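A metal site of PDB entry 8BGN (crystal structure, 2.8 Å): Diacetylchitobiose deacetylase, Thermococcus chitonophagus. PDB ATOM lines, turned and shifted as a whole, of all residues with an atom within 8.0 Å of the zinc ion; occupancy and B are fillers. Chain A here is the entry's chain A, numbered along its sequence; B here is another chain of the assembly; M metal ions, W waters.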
ATOM      1  N   GLU A  38      31.670   5.959   3.190  1.00  0.00           N
ATOM      2  CA  GLU A  38      31.182   7.234   2.599  1.00  0.00           C
ATOM      3  C   GLU A  38      30.202   6.930   1.466  1.00  0.00           C
ATOM      4  O   GLU A  38      30.478   6.089   0.617  1.00  0.00           O
ATOM      5  CB  GLU A  38      32.321   8.129   2.073  1.00  0.00           C
ATOM      6  CG  GLU A  38      33.357   7.444   1.192  1.00  0.00           C
ATOM      7  CD  GLU A  38      34.405   8.364   0.584  1.00  0.00           C
ATOM      8  OE1 GLU A  38      34.492   9.528   1.037  1.00  0.00           O
ATOM      9  OE2 GLU A  38      35.130   7.913  -0.363  1.00  0.00           O
ATOM     10  N   PRO A  39      29.054   7.653   1.404  1.00  0.00           N
ATOM     11  CA  PRO A  39      28.132   7.542   0.271  1.00  0.00           C
ATOM     12  C   PRO A  39      28.712   7.982  -1.091  1.00  0.00           C
ATOM     13  O   PRO A  39      28.403   7.309  -2.071  1.00  0.00           O
ATOM     14  CB  PRO A  39      26.960   8.454   0.637  1.00  0.00           C
ATOM     15  CG  PRO A  39      27.091   8.729   2.118  1.00  0.00           C
ATOM     16  CD  PRO A  39      28.554   8.580   2.434  1.00  0.00           C
ATOM     17  N   HIS A  40      29.460   9.099  -1.137  1.00  0.00           N
ATOM     18  CA  HIS A  40      30.084   9.646  -2.371  1.00  0.00           C
ATOM     19  C   HIS A  40      31.573   9.833  -2.151  1.00  0.00           C
ATOM     20  O   HIS A  40      32.056   9.976  -1.023  1.00  0.00           O
ATOM     21  CB  HIS A  40      29.427  10.988  -2.776  1.00  0.00           C
ATOM     22  CG  HIS A  40      27.945  10.913  -2.849  1.00  0.00           C
ATOM     23  ND1 HIS A  40      27.123  11.473  -1.901  1.00  0.00           N
ATOM     24  CD2 HIS A  40      27.134  10.280  -3.738  1.00  0.00           C
ATOM     25  CE1 HIS A  40      25.863  11.219  -2.200  1.00  0.00           C
ATOM     26  NE2 HIS A  40      25.842  10.483  -3.328  1.00  0.00           N
ATOM     27  N   PRO A  41      32.388   9.904  -3.217  1.00  0.00           N
ATOM     28  CA  PRO A  41      33.762  10.371  -3.090  1.00  0.00           C
ATOM     29  C   PRO A  41      33.747  11.787  -2.504  1.00  0.00           C
ATOM     30  O   PRO A  41      33.091  12.644  -3.077  1.00  0.00           O
ATOM     31  CB  PRO A  41      34.321  10.344  -4.521  1.00  0.00           C
ATOM     32  CG  PRO A  41      33.367   9.471  -5.289  1.00  0.00           C
ATOM     33  CD  PRO A  41      32.027   9.590  -4.599  1.00  0.00           C
ATOM     34  N   ASP A  42      34.405  11.960  -1.368  1.00  0.00           N
ATOM     35  CA  ASP A  42      34.656  13.255  -0.683  1.00  0.00           C
ATOM     36  C   ASP A  42      33.937  13.304   0.675  1.00  0.00           C
ATOM     37  O   ASP A  42      34.185  14.247   1.389  1.00  0.00           O
ATOM     38  CB  ASP A  42      34.319  14.479  -1.548  1.00  0.00           C
ATOM     39  CG  ASP A  42      32.860  14.861  -1.742  1.00  0.00           C
ATOM     40  OD1 ASP A  42      31.952  14.267  -1.087  1.00  0.00           O
ATOM     41  OD2 ASP A  42      32.646  15.754  -2.565  1.00  0.00           O
ATOM     42  N   ASP A  43      33.098  12.327   1.003  1.00  0.00           N
ATOM     43  CA  ASP A  43      32.255  12.400   2.219  1.00  0.00           C
ATOM     44  C   ASP A  43      33.087  12.078   3.469  1.00  0.00           C
ATOM     45  O   ASP A  43      32.850  12.724   4.520  1.00  0.00           O
ATOM     46  CB  ASP A  43      31.038  11.479   2.103  1.00  0.00           C
ATOM     47  CG  ASP A  43      29.853  12.218   1.562  1.00  0.00           C
ATOM     48  OD1 ASP A  43      29.727  13.416   1.892  1.00  0.00           O
ATOM     49  OD2 ASP A  43      29.070  11.580   0.788  1.00  0.00           O
ATOM     50  N   CYS A  44      33.992  11.103   3.398  1.00  0.00           N
ATOM     51  CA  CYS A  44      34.921  10.775   4.513  1.00  0.00           C
ATOM     52  C   CYS A  44      35.738  12.017   4.867  1.00  0.00           C
ATOM     53  O   CYS A  44      35.820  12.360   6.076  1.00  0.00           O
ATOM     54  CB  CYS A  44      35.841   9.616   4.165  1.00  0.00           C
ATOM     55  SG  CYS A  44      35.032   8.030   4.495  1.00  0.00           S
ATOM     56  N   ILE A  46      35.204  15.256   4.123  1.00  0.00           N
ATOM     57  CA  ILE A  46      34.353  16.429   4.524  1.00  0.00           C
ATOM     58  C   ILE A  46      33.815  16.232   5.944  1.00  0.00           C
ATOM     59  O   ILE A  46      33.703  17.225   6.686  1.00  0.00           O
ATOM     60  CB  ILE A  46      33.204  16.705   3.506  1.00  0.00           C
ATOM     61  CG1 ILE A  46      33.743  17.272   2.197  1.00  0.00           C
ATOM     62  CG2 ILE A  46      32.147  17.623   4.095  1.00  0.00           C
ATOM     63  CD1 ILE A  46      32.764  17.187   1.040  1.00  0.00           C
ATOM     64  N   THR A  68      29.188   4.766  -3.835  1.00  0.00           N
ATOM     65  CA  THR A  68      28.805   5.173  -5.200  1.00  0.00           C
ATOM     66  C   THR A  68      30.007   5.734  -5.934  1.00  0.00           C
ATOM     67  O   THR A  68      31.068   5.908  -5.320  1.00  0.00           O
ATOM     68  CB  THR A  68      27.652   6.176  -5.200  1.00  0.00           C
ATOM     69  OG1 THR A  68      28.167   7.423  -4.777  1.00  0.00           O
ATOM     70  CG2 THR A  68      26.484   5.762  -4.319  1.00  0.00           C
ATOM     71  N   ARG A  88      36.621  11.532 -10.243  1.00  0.00           N
ATOM     72  CA  ARG A  88      36.386  11.525  -8.789  1.00  0.00           C
ATOM     73  C   ARG A  88      37.111  10.338  -8.161  1.00  0.00           C
ATOM     74  O   ARG A  88      37.380  10.415  -6.963  1.00  0.00           O
ATOM     75  CB  ARG A  88      34.895  11.567  -8.462  1.00  0.00           C
ATOM     76  CG  ARG A  88      34.223  12.825  -8.963  1.00  0.00           C
ATOM     77  CD  ARG A  88      32.784  12.893  -8.507  1.00  0.00           C
ATOM     78  NE  ARG A  88      32.647  13.120  -7.086  1.00  0.00           N
ATOM     79  CZ  ARG A  88      31.511  13.400  -6.470  1.00  0.00           C
ATOM     80  NH1 ARG A  88      30.379  13.463  -7.153  1.00  0.00           N
ATOM     81  NH2 ARG A  88      31.496  13.609  -5.169  1.00  0.00           N
ATOM     82  N   ASP A 111      25.671   6.937  -8.182  1.00  0.00           N
ATOM     83  CA  ASP A 111      25.200   8.161  -7.484  1.00  0.00           C
ATOM     84  C   ASP A 111      23.695   8.348  -7.774  1.00  0.00           C
ATOM     85  O   ASP A 111      23.326   8.336  -8.940  1.00  0.00           O
ATOM     86  CB  ASP A 111      26.087   9.338  -7.953  1.00  0.00           C
ATOM     87  CG  ASP A 111      25.880  10.692  -7.298  1.00  0.00           C
ATOM     88  OD1 ASP A 111      24.978  10.829  -6.431  1.00  0.00           O
ATOM     89  OD2 ASP A 111      26.636  11.614  -7.678  1.00  0.00           O
ATOM     90  N   GLU A 146      18.218  15.656   6.099  1.00  0.00           N
ATOM     91  CA  GLU A 146      19.112  15.047   5.067  1.00  0.00           C
ATOM     92  C   GLU A 146      18.235  14.563   3.912  1.00  0.00           C
ATOM     93  O   GLU A 146      17.517  13.557   4.087  1.00  0.00           O
ATOM     94  CB  GLU A 146      19.947  13.939   5.685  1.00  0.00           C
ATOM     95  CG  GLU A 146      20.986  13.394   4.719  1.00  0.00           C
ATOM     96  CD  GLU A 146      21.864  14.417   4.038  1.00  0.00           C
ATOM     97  OE1 GLU A 146      22.668  15.079   4.725  1.00  0.00           O
ATOM     98  OE2 GLU A 146      21.742  14.566   2.820  1.00  0.00           O
ATOM     99  N   HIS A 148      19.402  13.865   0.694  1.00  0.00           N
ATOM    100  CA  HIS A 148      20.190  12.959  -0.184  1.00  0.00           C
ATOM    101  C   HIS A 148      19.916  11.498   0.184  1.00  0.00           C
ATOM    102  O   HIS A 148      20.325  11.022   1.248  1.00  0.00           O
ATOM    103  CB  HIS A 148      21.690  13.251  -0.148  1.00  0.00           C
ATOM    104  CG  HIS A 148      22.295  13.008  -1.479  1.00  0.00           C
ATOM    105  ND1 HIS A 148      22.169  11.784  -2.106  1.00  0.00           N
ATOM    106  CD2 HIS A 148      22.941  13.849  -2.313  1.00  0.00           C
ATOM    107  CE1 HIS A 148      22.741  11.864  -3.286  1.00  0.00           C
ATOM    108  NE2 HIS A 148      23.230  13.119  -3.455  1.00  0.00           N
ATOM    109  N   ASP A 150      21.049   8.644  -0.986  1.00  0.00           N
ATOM    110  CA  ASP A 150      22.314   7.864  -0.840  1.00  0.00           C
ATOM    111  C   ASP A 150      22.864   7.999   0.596  1.00  0.00           C
ATOM    112  O   ASP A 150      23.332   7.005   1.133  1.00  0.00           O
ATOM    113  CB  ASP A 150      23.349   8.297  -1.873  1.00  0.00           C
ATOM    114  CG  ASP A 150      23.074   7.974  -3.340  1.00  0.00           C
ATOM    115  OD1 ASP A 150      22.118   7.233  -3.635  1.00  0.00           O
ATOM    116  OD2 ASP A 150      23.838   8.478  -4.203  1.00  0.00           O
ATOM    117  N   HIS A 151      22.795   9.180   1.207  1.00  0.00           N
ATOM    118  CA  HIS A 151      23.262   9.390   2.598  1.00  0.00           C
ATOM    119  C   HIS A 151      22.447   8.569   3.590  1.00  0.00           C
ATOM    120  O   HIS A 151      23.045   7.721   4.283  1.00  0.00           O
ATOM    121  CB  HIS A 151      23.248  10.875   2.958  1.00  0.00           C
ATOM    122  CG  HIS A 151      24.514  11.558   2.571  1.00  0.00           C
ATOM    123  ND1 HIS A 151      25.315  12.193   3.496  1.00  0.00           N
ATOM    124  CD2 HIS A 151      25.124  11.659   1.359  1.00  0.00           C
ATOM    125  CE1 HIS A 151      26.377  12.669   2.847  1.00  0.00           C
ATOM    126  NE2 HIS A 151      26.289  12.353   1.533  1.00  0.00           N
ATOM    127  N   THR A 154      23.090   4.733   3.104  1.00  0.00           N
ATOM    128  CA  THR A 154      24.441   4.330   3.579  1.00  0.00           C
ATOM    129  C   THR A 154      24.443   4.107   5.084  1.00  0.00           C
ATOM    130  O   THR A 154      24.968   3.058   5.502  1.00  0.00           O
ATOM    131  CB  THR A 154      25.482   5.394   3.260  1.00  0.00           C
ATOM    132  OG1 THR A 154      25.440   5.630   1.851  1.00  0.00           O
ATOM    133  CG2 THR A 154      26.867   4.949   3.669  1.00  0.00           C
ATOM    134  N   TYR A 190      29.419   9.823  12.034  1.00  0.00           N
ATOM    135  CA  TYR A 190      29.862  11.178  11.625  1.00  0.00           C
ATOM    136  C   TYR A 190      28.675  11.868  10.971  1.00  0.00           C
ATOM    137  O   TYR A 190      27.598  11.290  10.981  1.00  0.00           O
ATOM    138  CB  TYR A 190      31.161  11.096  10.834  1.00  0.00           C
ATOM    139  CG  TYR A 190      31.091  10.536   9.443  1.00  0.00           C
ATOM    140  CD1 TYR A 190      31.186   9.163   9.228  1.00  0.00           C
ATOM    141  CD2 TYR A 190      31.046  11.364   8.337  1.00  0.00           C
ATOM    142  CE1 TYR A 190      31.171   8.633   7.952  1.00  0.00           C
ATOM    143  CE2 TYR A 190      31.017  10.838   7.061  1.00  0.00           C
ATOM    144  CZ  TYR A 190      31.068   9.471   6.869  1.00  0.00           C
ATOM    145  OH  TYR A 190      31.105   8.924   5.627  1.00  0.00           O
ATOM    146  N   TYR A 191      28.847  13.109  10.535  1.00  0.00           N
ATOM    147  CA  TYR A 191      27.729  13.943  10.041  1.00  0.00           C
ATOM    148  C   TYR A 191      26.521  13.818  10.987  1.00  0.00           C
ATOM    149  O   TYR A 191      25.399  13.556  10.492  1.00  0.00           O
ATOM    150  CB  TYR A 191      27.289  13.503   8.645  1.00  0.00           C
ATOM    151  CG  TYR A 191      28.201  13.839   7.495  1.00  0.00           C
ATOM    152  CD1 TYR A 191      28.928  15.024   7.435  1.00  0.00           C
ATOM    153  CD2 TYR A 191      28.252  12.992   6.397  1.00  0.00           C
ATOM    154  CE1 TYR A 191      29.710  15.335   6.315  1.00  0.00           C
ATOM    155  CE2 TYR A 191      29.026  13.282   5.284  1.00  0.00           C
ATOM    156  CZ  TYR A 191      29.738  14.467   5.237  1.00  0.00           C
ATOM    157  OH  TYR A 191      30.504  14.712   4.132  1.00  0.00           O
ATOM    158  N   HIS B 259      21.500  19.048   3.217  1.00  0.00           N
ATOM    159  CA  HIS B 259      22.627  18.112   3.054  1.00  0.00           C
ATOM    160  C   HIS B 259      23.720  18.438   4.085  1.00  0.00           C
ATOM    161  O   HIS B 259      24.252  19.580   4.039  1.00  0.00           O
ATOM    162  CB  HIS B 259      23.101  18.139   1.609  1.00  0.00           C
ATOM    163  CG  HIS B 259      24.128  17.118   1.276  1.00  0.00           C
ATOM    164  ND1 HIS B 259      23.900  15.758   1.473  1.00  0.00           N
ATOM    165  CD2 HIS B 259      25.380  17.261   0.769  1.00  0.00           C
ATOM    166  CE1 HIS B 259      24.969  15.105   1.063  1.00  0.00           C
ATOM    167  NE2 HIS B 259      25.907  16.001   0.624  1.00  0.00           N
ATOM    168  N   ILE B 260      24.004  17.452   4.952  1.00  0.00           N
ATOM    169  CA  ILE B 260      25.168  17.340   5.903  1.00  0.00           C
ATOM    170  C   ILE B 260      25.282  18.614   6.738  1.00  0.00           C
ATOM    171  O   ILE B 260      26.407  19.108   6.920  1.00  0.00           O
ATOM    172  CB  ILE B 260      26.487  17.000   5.165  1.00  0.00           C
ATOM    173  CG1 ILE B 260      26.853  18.002   4.069  1.00  0.00           C
ATOM    174  CG2 ILE B 260      26.450  15.590   4.610  1.00  0.00           C
ATOM    175  CD1 ILE B 260      28.313  18.013   3.716  1.00  0.00           C
HETATM  176 ZN    ZN M   1      27.689  12.665  -0.304  1.00  0.00          ZN
HETATM  177  O   HOH W   1      28.338  15.102  -0.794  1.00  0.00           O
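Water W1 lies within hydrogen-bond range of NE2 of His 259 of chain B (3.0 Å) and OD1 of Asp 43 (3.5 Å).
The zinc ion is bound by the side-chain carboxylate (OD2) of Asp 43. The zinc ion is bound by ND1 of His 40 (2.1 Å). The zinc ion is bound by NE2 of His 151 (2.3 Å). The zinc ion is bound by water W1, 2.6 Å away.
NE2 of His 259 of chain B touches the zinc ion, at 3.9 Å. Within 4 Å of the zinc ion: His 40, Asp 43, His 151 and His 259 of chain B. The nearest printed residue that does not touch the zinc ion is Pro 39 (4.4 Å).
The side-chain carboxylate (OE1) of Glu 38 lies within hydrogen-bond range of the backbone NH (N) of Asp 43 (3.1 Å). A ring nitrogen (NE2) of His 40 lies within hydrogen-bond range of the side-chain carboxylate (OD2) of Asp 150 (3.0 Å). The side-chain hydroxyl (OH) of Tyr 191 is in hydrogen-bond range of the side-chain carboxylate (OD1) of Asp 43 (2.7 Å). NE2 of His 40 is in hydrogen-bond range of OD1 of Asp 111. OE2 of Glu 146 is in hydrogen-bond range of ND1 of His 259 of chain B, at 2.8 Å.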
